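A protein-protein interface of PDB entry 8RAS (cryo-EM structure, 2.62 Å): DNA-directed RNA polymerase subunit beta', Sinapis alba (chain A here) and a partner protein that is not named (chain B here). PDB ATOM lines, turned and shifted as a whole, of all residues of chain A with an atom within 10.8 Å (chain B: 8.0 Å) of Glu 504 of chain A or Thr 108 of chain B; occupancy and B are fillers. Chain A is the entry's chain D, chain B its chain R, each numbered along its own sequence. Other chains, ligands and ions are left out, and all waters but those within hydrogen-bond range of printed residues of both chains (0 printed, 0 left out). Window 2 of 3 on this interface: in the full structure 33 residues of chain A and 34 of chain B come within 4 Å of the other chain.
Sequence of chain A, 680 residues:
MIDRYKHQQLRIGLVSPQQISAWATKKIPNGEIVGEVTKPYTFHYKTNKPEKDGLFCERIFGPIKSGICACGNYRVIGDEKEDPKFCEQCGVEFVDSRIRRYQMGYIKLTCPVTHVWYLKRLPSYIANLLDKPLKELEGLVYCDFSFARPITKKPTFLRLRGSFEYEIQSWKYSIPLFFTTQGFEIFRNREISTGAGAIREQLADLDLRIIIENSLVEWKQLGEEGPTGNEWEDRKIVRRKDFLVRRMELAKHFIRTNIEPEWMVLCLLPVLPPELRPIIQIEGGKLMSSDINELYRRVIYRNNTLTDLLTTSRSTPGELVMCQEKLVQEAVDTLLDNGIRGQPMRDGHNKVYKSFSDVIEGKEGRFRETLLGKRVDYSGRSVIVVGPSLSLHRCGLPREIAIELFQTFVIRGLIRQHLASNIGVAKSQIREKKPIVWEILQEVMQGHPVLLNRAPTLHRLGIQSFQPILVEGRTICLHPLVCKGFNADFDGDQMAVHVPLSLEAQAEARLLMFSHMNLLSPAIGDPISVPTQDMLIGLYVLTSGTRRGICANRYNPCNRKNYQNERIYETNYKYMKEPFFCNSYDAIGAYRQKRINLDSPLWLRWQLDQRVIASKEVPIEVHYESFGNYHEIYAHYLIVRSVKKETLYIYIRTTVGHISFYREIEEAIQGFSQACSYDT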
ATOM      1  N   HIS A 448      -1.805 -24.295  -7.750  1.00  0.00           N
ATOM      2  CA  HIS A 448      -1.453 -24.779  -9.079  1.00  0.00           C
ATOM      3  C   HIS A 448      -0.615 -26.039  -8.946  1.00  0.00           C
ATOM      4  O   HIS A 448       0.552 -25.957  -8.535  1.00  0.00           O
ATOM      5  CB  HIS A 448      -0.692 -23.707  -9.860  1.00  0.00           C
ATOM      6  CG  HIS A 448      -0.636 -23.956 -11.334  1.00  0.00           C
ATOM      7  ND1 HIS A 448      -0.720 -22.942 -12.263  1.00  0.00           N
ATOM      8  CD2 HIS A 448      -0.503 -25.102 -12.042  1.00  0.00           C
ATOM      9  CE1 HIS A 448      -0.642 -23.452 -13.478  1.00  0.00           C
ATOM     10  NE2 HIS A 448      -0.510 -24.761 -13.372  1.00  0.00           N
ATOM     11  N   PRO A 449      -1.147 -27.212  -9.273  1.00  0.00           N
ATOM     12  CA  PRO A 449      -0.394 -28.452  -9.077  1.00  0.00           C
ATOM     13  C   PRO A 449       0.671 -28.655 -10.146  1.00  0.00           C
ATOM     14  O   PRO A 449       0.681 -28.009 -11.194  1.00  0.00           O
ATOM     15  CB  PRO A 449      -1.475 -29.532  -9.168  1.00  0.00           C
ATOM     16  CG  PRO A 449      -2.495 -28.944 -10.076  1.00  0.00           C
ATOM     17  CD  PRO A 449      -2.490 -27.460  -9.827  1.00  0.00           C
ATOM     18  N   LEU A 451       3.237 -32.058 -11.875  1.00  0.00           N
ATOM     19  CA  LEU A 451       3.349 -33.499 -12.062  1.00  0.00           C
ATOM     20  C   LEU A 451       4.813 -33.905 -11.970  1.00  0.00           C
ATOM     21  O   LEU A 451       5.649 -33.402 -12.727  1.00  0.00           O
ATOM     22  CB  LEU A 451       2.763 -33.930 -13.407  1.00  0.00           C
ATOM     23  CG  LEU A 451       1.404 -33.360 -13.809  1.00  0.00           C
ATOM     24  CD1 LEU A 451       1.144 -33.612 -15.281  1.00  0.00           C
ATOM     25  CD2 LEU A 451       0.299 -33.962 -12.966  1.00  0.00           C
ATOM     26  N   SER A 465       0.797 -36.195  -8.952  1.00  0.00           N
ATOM     27  CA  SER A 465       0.602 -34.757  -8.852  1.00  0.00           C
ATOM     28  C   SER A 465       0.734 -34.312  -7.403  1.00  0.00           C
ATOM     29  O   SER A 465       0.254 -34.987  -6.488  1.00  0.00           O
ATOM     30  CB  SER A 465      -0.765 -34.350  -9.403  1.00  0.00           C
ATOM     31  OG  SER A 465      -0.776 -32.983  -9.769  1.00  0.00           O
ATOM     32  N   VAL A 499       4.027 -28.752 -15.592  1.00  0.00           N
ATOM     33  CA  VAL A 499       3.026 -27.797 -15.128  1.00  0.00           C
ATOM     34  C   VAL A 499       1.806 -27.906 -16.037  1.00  0.00           C
ATOM     35  O   VAL A 499       1.905 -27.607 -17.234  1.00  0.00           O
ATOM     36  CB  VAL A 499       3.573 -26.360 -15.119  1.00  0.00           C
ATOM     37  CG1 VAL A 499       2.444 -25.364 -14.928  1.00  0.00           C
ATOM     38  CG2 VAL A 499       4.606 -26.198 -14.028  1.00  0.00           C
ATOM     39  N   PRO A 500       0.651 -28.335 -15.529  1.00  0.00           N
ATOM     40  CA  PRO A 500      -0.580 -28.243 -16.324  1.00  0.00           C
ATOM     41  C   PRO A 500      -0.982 -26.787 -16.502  1.00  0.00           C
ATOM     42  O   PRO A 500      -1.075 -26.033 -15.532  1.00  0.00           O
ATOM     43  CB  PRO A 500      -1.609 -29.017 -15.492  1.00  0.00           C
ATOM     44  CG  PRO A 500      -0.813 -29.786 -14.484  1.00  0.00           C
ATOM     45  CD  PRO A 500       0.424 -28.995 -14.235  1.00  0.00           C
ATOM     46  N   LEU A 501      -1.221 -26.394 -17.752  1.00  0.00           N
ATOM     47  CA  LEU A 501      -1.469 -24.993 -18.074  1.00  0.00           C
ATOM     48  C   LEU A 501      -2.958 -24.661 -18.081  1.00  0.00           C
ATOM     49  O   LEU A 501      -3.404 -23.766 -17.356  1.00  0.00           O
ATOM     50  CB  LEU A 501      -0.837 -24.652 -19.427  1.00  0.00           C
ATOM     51  CG  LEU A 501       0.681 -24.809 -19.512  1.00  0.00           C
ATOM     52  CD1 LEU A 501       1.165 -24.510 -20.917  1.00  0.00           C
ATOM     53  CD2 LEU A 501       1.369 -23.911 -18.501  1.00  0.00           C
ATOM     54  N   SER A 502      -3.733 -25.365 -18.899  1.00  0.00           N
ATOM     55  CA  SER A 502      -5.151 -25.074 -19.021  1.00  0.00           C
ATOM     56  C   SER A 502      -5.904 -25.502 -17.764  1.00  0.00           C
ATOM     57  O   SER A 502      -5.423 -26.300 -16.958  1.00  0.00           O
ATOM     58  CB  SER A 502      -5.737 -25.770 -20.249  1.00  0.00           C
ATOM     59  OG  SER A 502      -5.961 -27.145 -19.994  1.00  0.00           O
ATOM     60  N   LEU A 503      -7.108 -24.946 -17.604  1.00  0.00           N
ATOM     61  CA  LEU A 503      -7.913 -25.232 -16.420  1.00  0.00           C
ATOM     62  C   LEU A 503      -8.330 -26.696 -16.364  1.00  0.00           C
ATOM     63  O   LEU A 503      -8.372 -27.290 -15.282  1.00  0.00           O
ATOM     64  CB  LEU A 503      -9.144 -24.329 -16.390  1.00  0.00           C
ATOM     65  CG  LEU A 503      -8.956 -22.935 -15.794  1.00  0.00           C
ATOM     66  CD1 LEU A 503     -10.147 -22.062 -16.132  1.00  0.00           C
ATOM     67  CD2 LEU A 503      -8.751 -23.009 -14.293  1.00  0.00           C
ATOM     68  N   GLU A 504      -8.665 -27.289 -17.512  1.00  0.00           N
ATOM     69  CA  GLU A 504      -9.063 -28.694 -17.528  1.00  0.00           C
ATOM     70  C   GLU A 504      -7.921 -29.596 -17.075  1.00  0.00           C
ATOM     71  O   GLU A 504      -8.138 -30.544 -16.310  1.00  0.00           O
ATOM     72  CB  GLU A 504      -9.560 -29.115 -18.917  1.00  0.00           C
ATOM     73  CG  GLU A 504     -10.525 -28.162 -19.647  1.00  0.00           C
ATOM     74  CD  GLU A 504      -9.933 -26.806 -19.987  1.00  0.00           C
ATOM     75  OE1 GLU A 504      -8.695 -26.708 -20.089  1.00  0.00           O
ATOM     76  OE2 GLU A 504     -10.708 -25.839 -20.145  1.00  0.00           O
ATOM     77  N   ALA A 505      -6.700 -29.320 -17.534  1.00  0.00           N
ATOM     78  CA  ALA A 505      -5.553 -30.113 -17.103  1.00  0.00           C
ATOM     79  C   ALA A 505      -5.290 -29.944 -15.612  1.00  0.00           C
ATOM     80  O   ALA A 505      -4.964 -30.915 -14.919  1.00  0.00           O
ATOM     81  CB  ALA A 505      -4.317 -29.732 -17.912  1.00  0.00           C
ATOM     82  N   GLN A 506      -5.419 -28.718 -15.102  1.00  0.00           N
ATOM     83  CA  GLN A 506      -5.236 -28.487 -13.672  1.00  0.00           C
ATOM     84  C   GLN A 506      -6.280 -29.236 -12.857  1.00  0.00           C
ATOM     85  O   GLN A 506      -5.963 -29.820 -11.814  1.00  0.00           O
ATOM     86  CB  GLN A 506      -5.299 -26.992 -13.373  1.00  0.00           C
ATOM     87  CG  GLN A 506      -4.165 -26.188 -13.962  1.00  0.00           C
ATOM     88  CD  GLN A 506      -4.213 -24.740 -13.535  1.00  0.00           C
ATOM     89  OE1 GLN A 506      -4.426 -24.437 -12.363  1.00  0.00           O
ATOM     90  NE2 GLN A 506      -4.022 -23.835 -14.486  1.00  0.00           N
ATOM     91  N   ALA A 507      -7.534 -29.225 -13.313  1.00  0.00           N
ATOM     92  CA  ALA A 507      -8.581 -29.971 -12.624  1.00  0.00           C
ATOM     93  C   ALA A 507      -8.302 -31.465 -12.659  1.00  0.00           C
ATOM     94  O   ALA A 507      -8.504 -32.164 -11.659  1.00  0.00           O
ATOM     95  CB  ALA A 507      -9.942 -29.664 -13.247  1.00  0.00           C
ATOM     96  N   GLU A 508      -7.839 -31.976 -13.801  1.00  0.00           N
ATOM     97  CA  GLU A 508      -7.498 -33.390 -13.901  1.00  0.00           C
ATOM     98  C   GLU A 508      -6.398 -33.753 -12.914  1.00  0.00           C
ATOM     99  O   GLU A 508      -6.493 -34.757 -12.199  1.00  0.00           O
ATOM    100  CB  GLU A 508      -7.057 -33.722 -15.326  1.00  0.00           C
ATOM    101  CG  GLU A 508      -8.179 -34.044 -16.286  1.00  0.00           C
ATOM    102  CD  GLU A 508      -7.666 -34.323 -17.681  1.00  0.00           C
ATOM    103  OE1 GLU A 508      -6.488 -34.012 -17.951  1.00  0.00           O
ATOM    104  OE2 GLU A 508      -8.434 -34.851 -18.510  1.00  0.00           O
ATOM    105  N   ALA A 509      -5.350 -32.929 -12.853  1.00  0.00           N
ATOM    106  CA  ALA A 509      -4.240 -33.199 -11.950  1.00  0.00           C
ATOM    107  C   ALA A 509      -4.678 -33.130 -10.493  1.00  0.00           C
ATOM    108  O   ALA A 509      -4.238 -33.936  -9.666  1.00  0.00           O
ATOM    109  CB  ALA A 509      -3.099 -32.219 -12.215  1.00  0.00           C
ATOM    110  N   ARG A 510      -5.545 -32.173 -10.157  1.00  0.00           N
ATOM    111  CA  ARG A 510      -5.956 -32.014  -8.767  1.00  0.00           C
ATOM    112  C   ARG A 510      -6.905 -33.123  -8.330  1.00  0.00           C
ATOM    113  O   ARG A 510      -6.817 -33.606  -7.196  1.00  0.00           O
ATOM    114  CB  ARG A 510      -6.607 -30.645  -8.566  1.00  0.00           C
ATOM    115  CG  ARG A 510      -6.903 -30.306  -7.114  1.00  0.00           C
ATOM    116  CD  ARG A 510      -5.632 -30.313  -6.284  1.00  0.00           C
ATOM    117  NE  ARG A 510      -5.889 -30.496  -4.860  1.00  0.00           N
ATOM    118  CZ  ARG A 510      -6.243 -31.645  -4.298  1.00  0.00           C
ATOM    119  NH1 ARG A 510      -6.406 -32.745  -5.014  1.00  0.00           N
ATOM    120  NH2 ARG A 510      -6.433 -31.692  -2.984  1.00  0.00           N
ATOM    121  N   LEU A 511      -7.818 -33.543  -9.207  1.00  0.00           N
ATOM    122  CA  LEU A 511      -8.893 -34.443  -8.817  1.00  0.00           C
ATOM    123  C   LEU A 511      -8.648 -35.899  -9.188  1.00  0.00           C
ATOM    124  O   LEU A 511      -9.457 -36.753  -8.810  1.00  0.00           O
ATOM    125  CB  LEU A 511     -10.216 -33.985  -9.446  1.00  0.00           C
ATOM    126  CG  LEU A 511     -10.662 -32.546  -9.184  1.00  0.00           C
ATOM    127  CD1 LEU A 511     -11.823 -32.172 -10.089  1.00  0.00           C
ATOM    128  CD2 LEU A 511     -11.038 -32.361  -7.731  1.00  0.00           C
ATOM    129  N   LEU A 512      -7.573 -36.215  -9.906  1.00  0.00           N
ATOM    130  CA  LEU A 512      -7.376 -37.597 -10.323  1.00  0.00           C
ATOM    131  C   LEU A 512      -5.990 -38.126  -9.980  1.00  0.00           C
ATOM    132  O   LEU A 512      -5.823 -39.328  -9.753  1.00  0.00           O
ATOM    133  CB  LEU A 512      -7.624 -37.735 -11.827  1.00  0.00           C
ATOM    134  CG  LEU A 512      -9.057 -37.526 -12.318  1.00  0.00           C
ATOM    135  CD1 LEU A 512      -9.094 -37.461 -13.834  1.00  0.00           C
ATOM    136  CD2 LEU A 512      -9.968 -38.625 -11.808  1.00  0.00           C
ATOM    137  N   MET A 513      -4.988 -37.250  -9.938  1.00  0.00           N
ATOM    138  CA  MET A 513      -3.602 -37.681  -9.856  1.00  0.00           C
ATOM    139  C   MET A 513      -2.938 -37.389  -8.517  1.00  0.00           C
ATOM    140  O   MET A 513      -1.784 -37.782  -8.324  1.00  0.00           O
ATOM    141  CB  MET A 513      -2.786 -37.037 -10.981  1.00  0.00           C
ATOM    142  CG  MET A 513      -3.221 -37.453 -12.372  1.00  0.00           C
ATOM    143  SD  MET A 513      -2.128 -36.821 -13.650  1.00  0.00           S
ATOM    144  CE  MET A 513      -0.600 -37.637 -13.207  1.00  0.00           C
ATOM    145  N   VAL B 100     -14.967 -34.239 -12.978  1.00  0.00           N
ATOM    146  CA  VAL B 100     -13.819 -33.412 -13.335  1.00  0.00           C
ATOM    147  C   VAL B 100     -14.167 -32.491 -14.496  1.00  0.00           C
ATOM    148  O   VAL B 100     -13.811 -31.306 -14.498  1.00  0.00           O
ATOM    149  CB  VAL B 100     -12.602 -34.299 -13.661  1.00  0.00           C
ATOM    150  CG1 VAL B 100     -11.449 -33.457 -14.174  1.00  0.00           C
ATOM    151  CG2 VAL B 100     -12.179 -35.086 -12.434  1.00  0.00           C
ATOM    152  N   ASN B 101     -14.871 -33.019 -15.501  1.00  0.00           N
ATOM    153  CA  ASN B 101     -15.247 -32.202 -16.650  1.00  0.00           C
ATOM    154  C   ASN B 101     -16.168 -31.058 -16.243  1.00  0.00           C
ATOM    155  O   ASN B 101     -15.998 -29.921 -16.700  1.00  0.00           O
ATOM    156  CB  ASN B 101     -15.913 -33.075 -17.712  1.00  0.00           C
ATOM    157  CG  ASN B 101     -14.911 -33.759 -18.614  1.00  0.00           C
ATOM    158  OD1 ASN B 101     -13.796 -33.276 -18.797  1.00  0.00           O
ATOM    159  ND2 ASN B 101     -15.302 -34.892 -19.180  1.00  0.00           N
ATOM    160  N   SER B 102     -17.150 -31.337 -15.383  1.00  0.00           N
ATOM    161  CA  SER B 102     -18.068 -30.291 -14.940  1.00  0.00           C
ATOM    162  C   SER B 102     -17.352 -29.241 -14.103  1.00  0.00           C
ATOM    163  O   SER B 102     -17.625 -28.041 -14.235  1.00  0.00           O
ATOM    164  CB  SER B 102     -19.224 -30.909 -14.157  1.00  0.00           C
ATOM    165  OG  SER B 102     -18.755 -31.561 -12.993  1.00  0.00           O
ATOM    166  N   VAL B 103     -16.429 -29.668 -13.237  1.00  0.00           N
ATOM    167  CA  VAL B 103     -15.662 -28.715 -12.442  1.00  0.00           C
ATOM    168  C   VAL B 103     -14.821 -27.825 -13.347  1.00  0.00           C
ATOM    169  O   VAL B 103     -14.743 -26.606 -13.147  1.00  0.00           O
ATOM    170  CB  VAL B 103     -14.796 -29.458 -11.407  1.00  0.00           C
ATOM    171  CG1 VAL B 103     -13.704 -28.550 -10.869  1.00  0.00           C
ATOM    172  CG2 VAL B 103     -15.659 -29.980 -10.273  1.00  0.00           C
ATOM    173  N   ALA B 104     -14.186 -28.416 -14.361  1.00  0.00           N
ATOM    174  CA  ALA B 104     -13.381 -27.629 -15.289  1.00  0.00           C
ATOM    175  C   ALA B 104     -14.240 -26.640 -16.067  1.00  0.00           C
ATOM    176  O   ALA B 104     -13.833 -25.494 -16.283  1.00  0.00           O
ATOM    177  CB  ALA B 104     -12.624 -28.552 -16.243  1.00  0.00           C
ATOM    178  N   ALA B 105     -15.431 -27.064 -16.496  1.00  0.00           N
ATOM    179  CA  ALA B 105     -16.320 -26.159 -17.220  1.00  0.00           C
ATOM    180  C   ALA B 105     -16.771 -25.000 -16.338  1.00  0.00           C
ATOM    181  O   ALA B 105     -16.813 -23.846 -16.785  1.00  0.00           O
ATOM    182  CB  ALA B 105     -17.526 -26.925 -17.759  1.00  0.00           C
ATOM    183  N   GLU B 106     -17.115 -25.288 -15.080  1.00  0.00           N
ATOM    184  CA  GLU B 106     -17.527 -24.225 -14.168  1.00  0.00           C
ATOM    185  C   GLU B 106     -16.384 -23.255 -13.897  1.00  0.00           C
ATOM    186  O   GLU B 106     -16.591 -22.036 -13.846  1.00  0.00           O
ATOM    187  CB  GLU B 106     -18.048 -24.828 -12.866  1.00  0.00           C
ATOM    188  CG  GLU B 106     -18.910 -23.883 -12.052  1.00  0.00           C
ATOM    189  CD  GLU B 106     -19.461 -24.535 -10.803  1.00  0.00           C
ATOM    190  OE1 GLU B 106     -19.549 -25.779 -10.771  1.00  0.00           O
ATOM    191  OE2 GLU B 106     -19.806 -23.805  -9.851  1.00  0.00           O
ATOM    192  N   ALA B 107     -15.166 -23.775 -13.721  1.00  0.00           N
ATOM    193  CA  ALA B 107     -14.011 -22.905 -13.525  1.00  0.00           C
ATOM    194  C   ALA B 107     -13.753 -22.047 -14.757  1.00  0.00           C
ATOM    195  O   ALA B 107     -13.393 -20.868 -14.639  1.00  0.00           O
ATOM    196  CB  ALA B 107     -12.777 -23.737 -13.181  1.00  0.00           C
ATOM    197  N   THR B 108     -13.921 -22.624 -15.948  1.00  0.00           N
ATOM    198  CA  THR B 108     -13.761 -21.851 -17.174  1.00  0.00           C
ATOM    199  C   THR B 108     -14.779 -20.721 -17.244  1.00  0.00           C
ATOM    200  O   THR B 108     -14.437 -19.591 -17.611  1.00  0.00           O
ATOM    201  CB  THR B 108     -13.887 -22.767 -18.390  1.00  0.00           C
ATOM    202  OG1 THR B 108     -12.794 -23.692 -18.408  1.00  0.00           O
ATOM    203  CG2 THR B 108     -13.875 -21.958 -19.675  1.00  0.00           C
ATOM    204  N   GLU B 109     -16.034 -21.006 -16.891  1.00  0.00           N
ATOM    205  CA  GLU B 109     -17.046 -19.953 -16.863  1.00  0.00           C
ATOM    206  C   GLU B 109     -16.679 -18.866 -15.859  1.00  0.00           C
ATOM    207  O   GLU B 109     -16.835 -17.671 -16.141  1.00  0.00           O
ATOM    208  CB  GLU B 109     -18.415 -20.542 -16.534  1.00  0.00           C
ATOM    209  CG  GLU B 109     -18.960 -21.481 -17.591  1.00  0.00           C
ATOM    210  CD  GLU B 109     -20.153 -22.272 -17.097  1.00  0.00           C
ATOM    211  OE1 GLU B 109     -20.572 -22.058 -15.939  1.00  0.00           O
ATOM    212  OE2 GLU B 109     -20.673 -23.109 -17.865  1.00  0.00           O
ATOM    213  N   TYR B 110     -16.193 -19.264 -14.679  1.00  0.00           N
ATOM    214  CA  TYR B 110     -15.760 -18.288 -13.683  1.00  0.00           C
ATOM    215  C   TYR B 110     -14.669 -17.384 -14.238  1.00  0.00           C
ATOM    216  O   TYR B 110     -14.704 -16.164 -14.045  1.00  0.00           O
ATOM    217  CB  TYR B 110     -15.252 -18.995 -12.427  1.00  0.00           C
ATOM    218  CG  TYR B 110     -16.320 -19.542 -11.510  1.00  0.00           C
ATOM    219  CD1 TYR B 110     -17.649 -19.594 -11.902  1.00  0.00           C
ATOM    220  CD2 TYR B 110     -15.993 -20.006 -10.244  1.00  0.00           C
ATOM    221  CE1 TYR B 110     -18.620 -20.097 -11.060  1.00  0.00           C
ATOM    222  CE2 TYR B 110     -16.955 -20.508  -9.397  1.00  0.00           C
ATOM    223  CZ  TYR B 110     -18.266 -20.552  -9.808  1.00  0.00           C
ATOM    224  OH  TYR B 110     -19.228 -21.053  -8.962  1.00  0.00           O
ATOM    225  N   VAL B 111     -13.686 -17.969 -14.924  1.00  0.00           N
ATOM    226  CA  VAL B 111     -12.574 -17.177 -15.443  1.00  0.00           C
ATOM    227  C   VAL B 111     -13.047 -16.239 -16.546  1.00  0.00           C
ATOM    228  O   VAL B 111     -12.639 -15.074 -16.602  1.00  0.00           O
ATOM    229  CB  VAL B 111     -11.439 -18.097 -15.925  1.00  0.00           C
ATOM    230  CG1 VAL B 111     -10.399 -17.301 -16.691  1.00  0.00           C
ATOM    231  CG2 VAL B 111     -10.798 -18.788 -14.746  1.00  0.00           C
ATOM    232  N   GLU B 112     -13.909 -16.723 -17.443  1.00  0.00           N
ATOM    233  CA  GLU B 112     -14.393 -15.861 -18.518  1.00  0.00           C
ATOM    234  C   GLU B 112     -15.225 -14.704 -17.977  1.00  0.00           C
ATOM    235  O   GLU B 112     -15.123 -13.576 -18.473  1.00  0.00           O
ATOM    236  CB  GLU B 112     -15.196 -16.668 -19.539  1.00  0.00           C
ATOM    237  CG  GLU B 112     -14.470 -17.882 -20.085  1.00  0.00           C
ATOM    238  CD  GLU B 112     -14.521 -17.965 -21.595  1.00  0.00           C
ATOM    239  OE1 GLU B 112     -14.046 -17.020 -22.259  1.00  0.00           O
ATOM    240  OE2 GLU B 112     -15.037 -18.975 -22.118  1.00  0.00           O
ATOM    241  N   LYS B 113     -16.055 -14.959 -16.962  1.00  0.00           N
ATOM    242  CA  LYS B 113     -16.912 -13.896 -16.439  1.00  0.00           C
ATOM    243  C   LYS B 113     -16.100 -12.820 -15.728  1.00  0.00           C
ATOM    244  O   LYS B 113     -16.274 -11.625 -15.990  1.00  0.00           O
ATOM    245  CB  LYS B 113     -17.968 -14.484 -15.505  1.00  0.00           C
ATOM    246  CG  LYS B 113     -19.335 -14.637 -16.151  1.00  0.00           C
ATOM    247  CD  LYS B 113     -20.123 -15.771 -15.521  1.00  0.00           C
ATOM    248  CE  LYS B 113     -21.071 -16.401 -16.529  1.00  0.00           C
ATOM    249  NZ  LYS B 113     -20.334 -16.972 -17.690  1.00  0.00           N
ATOM    250  N   ASN B 114     -15.204 -13.220 -14.824  1.00  0.00           N
ATOM    251  CA  ASN B 114     -14.388 -12.284 -14.043  1.00  0.00           C
ATOM    252  C   ASN B 114     -12.933 -12.732 -14.141  1.00  0.00           C
ATOM    253  O   ASN B 114     -12.450 -13.492 -13.298  1.00  0.00           O
ATOM    254  CB  ASN B 114     -14.860 -12.219 -12.596  1.00  0.00           C
ATOM    255  CG  ASN B 114     -16.336 -12.524 -12.450  1.00  0.00           C
ATOM    256  OD1 ASN B 114     -16.719 -13.644 -12.115  1.00  0.00           O
ATOM    257  ND2 ASN B 114     -17.175 -11.527 -12.704  1.00  0.00           N
ATOM    258  N   TYR B 118      -8.945 -13.981 -10.546  1.00  0.00           N
ATOM    259  CA  TYR B 118      -8.329 -15.285 -10.376  1.00  0.00           C
ATOM    260  C   TYR B 118      -6.881 -15.252 -10.844  1.00  0.00           C
ATOM    261  O   TYR B 118      -6.433 -14.312 -11.506  1.00  0.00           O
ATOM    262  CB  TYR B 118      -9.112 -16.360 -11.138  1.00  0.00           C
ATOM    263  CG  TYR B 118     -10.572 -16.414 -10.761  1.00  0.00           C
ATOM    264  CD1 TYR B 118     -10.977 -16.977  -9.561  1.00  0.00           C
ATOM    265  CD2 TYR B 118     -11.542 -15.895 -11.601  1.00  0.00           C
ATOM    266  CE1 TYR B 118     -12.308 -17.026  -9.212  1.00  0.00           C
ATOM    267  CE2 TYR B 118     -12.877 -15.939 -11.259  1.00  0.00           C
ATOM    268  CZ  TYR B 118     -13.253 -16.504 -10.063  1.00  0.00           C
ATOM    269  OH  TYR B 118     -14.583 -16.551  -9.717  1.00  0.00           O
ATOM    270  N   ALA B 124      -9.578 -20.448  -9.636  1.00  0.00           N
ATOM    271  CA  ALA B 124     -10.918 -20.730 -10.143  1.00  0.00           C
ATOM    272  C   ALA B 124     -11.400 -22.113  -9.725  1.00  0.00           C
ATOM    273  O   ALA B 124     -12.561 -22.278  -9.334  1.00  0.00           O
ATOM    274  CB  ALA B 124     -10.940 -20.598 -11.662  1.00  0.00           C
ATOM    275  N   ILE B 125     -10.531 -23.121  -9.812  1.00  0.00           N
ATOM    276  CA  ILE B 125     -10.931 -24.475  -9.442  1.00  0.00           C
ATOM    277  C   ILE B 125     -11.207 -24.561  -7.947  1.00  0.00           C
ATOM    278  O   ILE B 125     -12.158 -25.222  -7.512  1.00  0.00           O
ATOM    279  CB  ILE B 125      -9.858 -25.484  -9.887  1.00  0.00           C
ATOM    280  CG1 ILE B 125      -9.646 -25.390 -11.397  1.00  0.00           C
ATOM    281  CG2 ILE B 125     -10.253 -26.898  -9.493  1.00  0.00           C
ATOM    282  CD1 ILE B 125      -8.572 -26.303 -11.917  1.00  0.00           C
ATOM    283  N   VAL B 128     -14.551 -23.030  -7.383  1.00  0.00           N
ATOM    284  CA  VAL B 128     -15.614 -23.944  -7.794  1.00  0.00           C
ATOM    285  C   VAL B 128     -15.841 -25.006  -6.729  1.00  0.00           C
ATOM    286  O   VAL B 128     -16.983 -25.315  -6.367  1.00  0.00           O
ATOM    287  CB  VAL B 128     -15.278 -24.576  -9.157  1.00  0.00           C
ATOM    288  CG1 VAL B 128     -16.168 -25.774  -9.427  1.00  0.00           C
ATOM    289  CG2 VAL B 128     -15.418 -23.552 -10.261  1.00  0.00           C
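The side-chain hydroxyl (OG1) of Thr 108 of chain B is in hydrogen-bond range of the side-chain carboxylate (OE2) of Glu 504 of chain A (3.5 Å).
O of Leu 501 of chain A sits at hydrogen-bond distance from NE2 of Gln 506 of chain A (2.9 Å).
The side-chain carboxylate (OE1) of Glu 504 of chain A is in hydrogen-bond range of the side-chain hydroxyl (OG) of Ser 502 of chain A (2.8 Å).
The side-chain hydroxyl (OG1) of Thr 108 of chain B lies within hydrogen-bond range of the backbone carbonyl oxygen (O) of Ala 104 of chain B, at 3.0 Å.
Leu 503 of chain A touches Ala 107 of chain B.
CA of Thr 108 of chain B touches CD1 of Leu 503 of chain A (3.8 Å).
Leu 503 of chain A touches Val 111 of chain B.
O of Leu 503 of chain A touches CD1 of Ile 125 of chain B, 3.5 Å away.
CB of Ala 104 of chain B touches CA of Glu 504 of chain A, 3.8 Å away.
Gln 506 of chain A touches Ile 125 of chain B.
Ala 507 of chain A touches Ile 125 of chain B.
CG1 of Val 100 of chain B touches N of Glu 508 of chain A, at 3.9 Å.
Val 100 of chain B touches Leu 511 of chain A.
CG of Leu 512 of chain A touches CG2 of Val 100 of chain B, 3.96 Å away.
Of chain B, only Ala 104 and Thr 108 come within 4 Å of Glu 504 of chain A.
Of the printed residues of chain B, Gln 506 of chain A touches Ile 125.
Printed residues of chain A within 4 Å of Val 100 of chain B: Glu 508 (3.9 Å), Leu 511 (3.7 Å) and Leu 512 (3.96 Å).
Asn 101 of chain B touches none of the printed residues of chain A.
Of chain A, only Glu 504 comes within 4 Å of Ala 104 of chain B.
Ala 107 of chain B touches just one residue of chain A: Leu 503.
Thr 108 of chain B touches just these residues of chain A: Leu 503 (3.8 Å) and Glu 504 (3.5 Å).
Val 111 of chain B touches just one residue of chain A: Leu 503.
Printed residues of chain A within 4 Å of Ile 125 of chain B: Leu 503 (3.5 Å), Gln 506 (3.6 Å) and Ala 507 (3.4 Å).
The nearest residue of chain B that does not touch Glu 504 of chain A is Val 100 of chain B (4.9 Å).
The nearest printed residue of chain B that does not touch Glu 508 of chain A is Asn 101 of chain B (5.6 Å).
Of the 19 printed residues of chain A, 7 touch a printed residue of chain B.
Printed residues of chain A that touch a printed residue of chain B: Leu 503, Glu 504, Gln 506, Ala 507, Glu 508, Leu 511 and Leu 512.
Along chain A the printed residues that touch a printed residue of chain B span positions 503 to 512.
Hydrophobic or aromatic side chains of chain B that line the printed part of chain A: Val 100, Ala 104, Val 111 and Ile 125.
Among the printed residues, no Asp or Glu carboxylate lies within 4 Å of a Lys or Arg side-chain nitrogen of the other chain.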
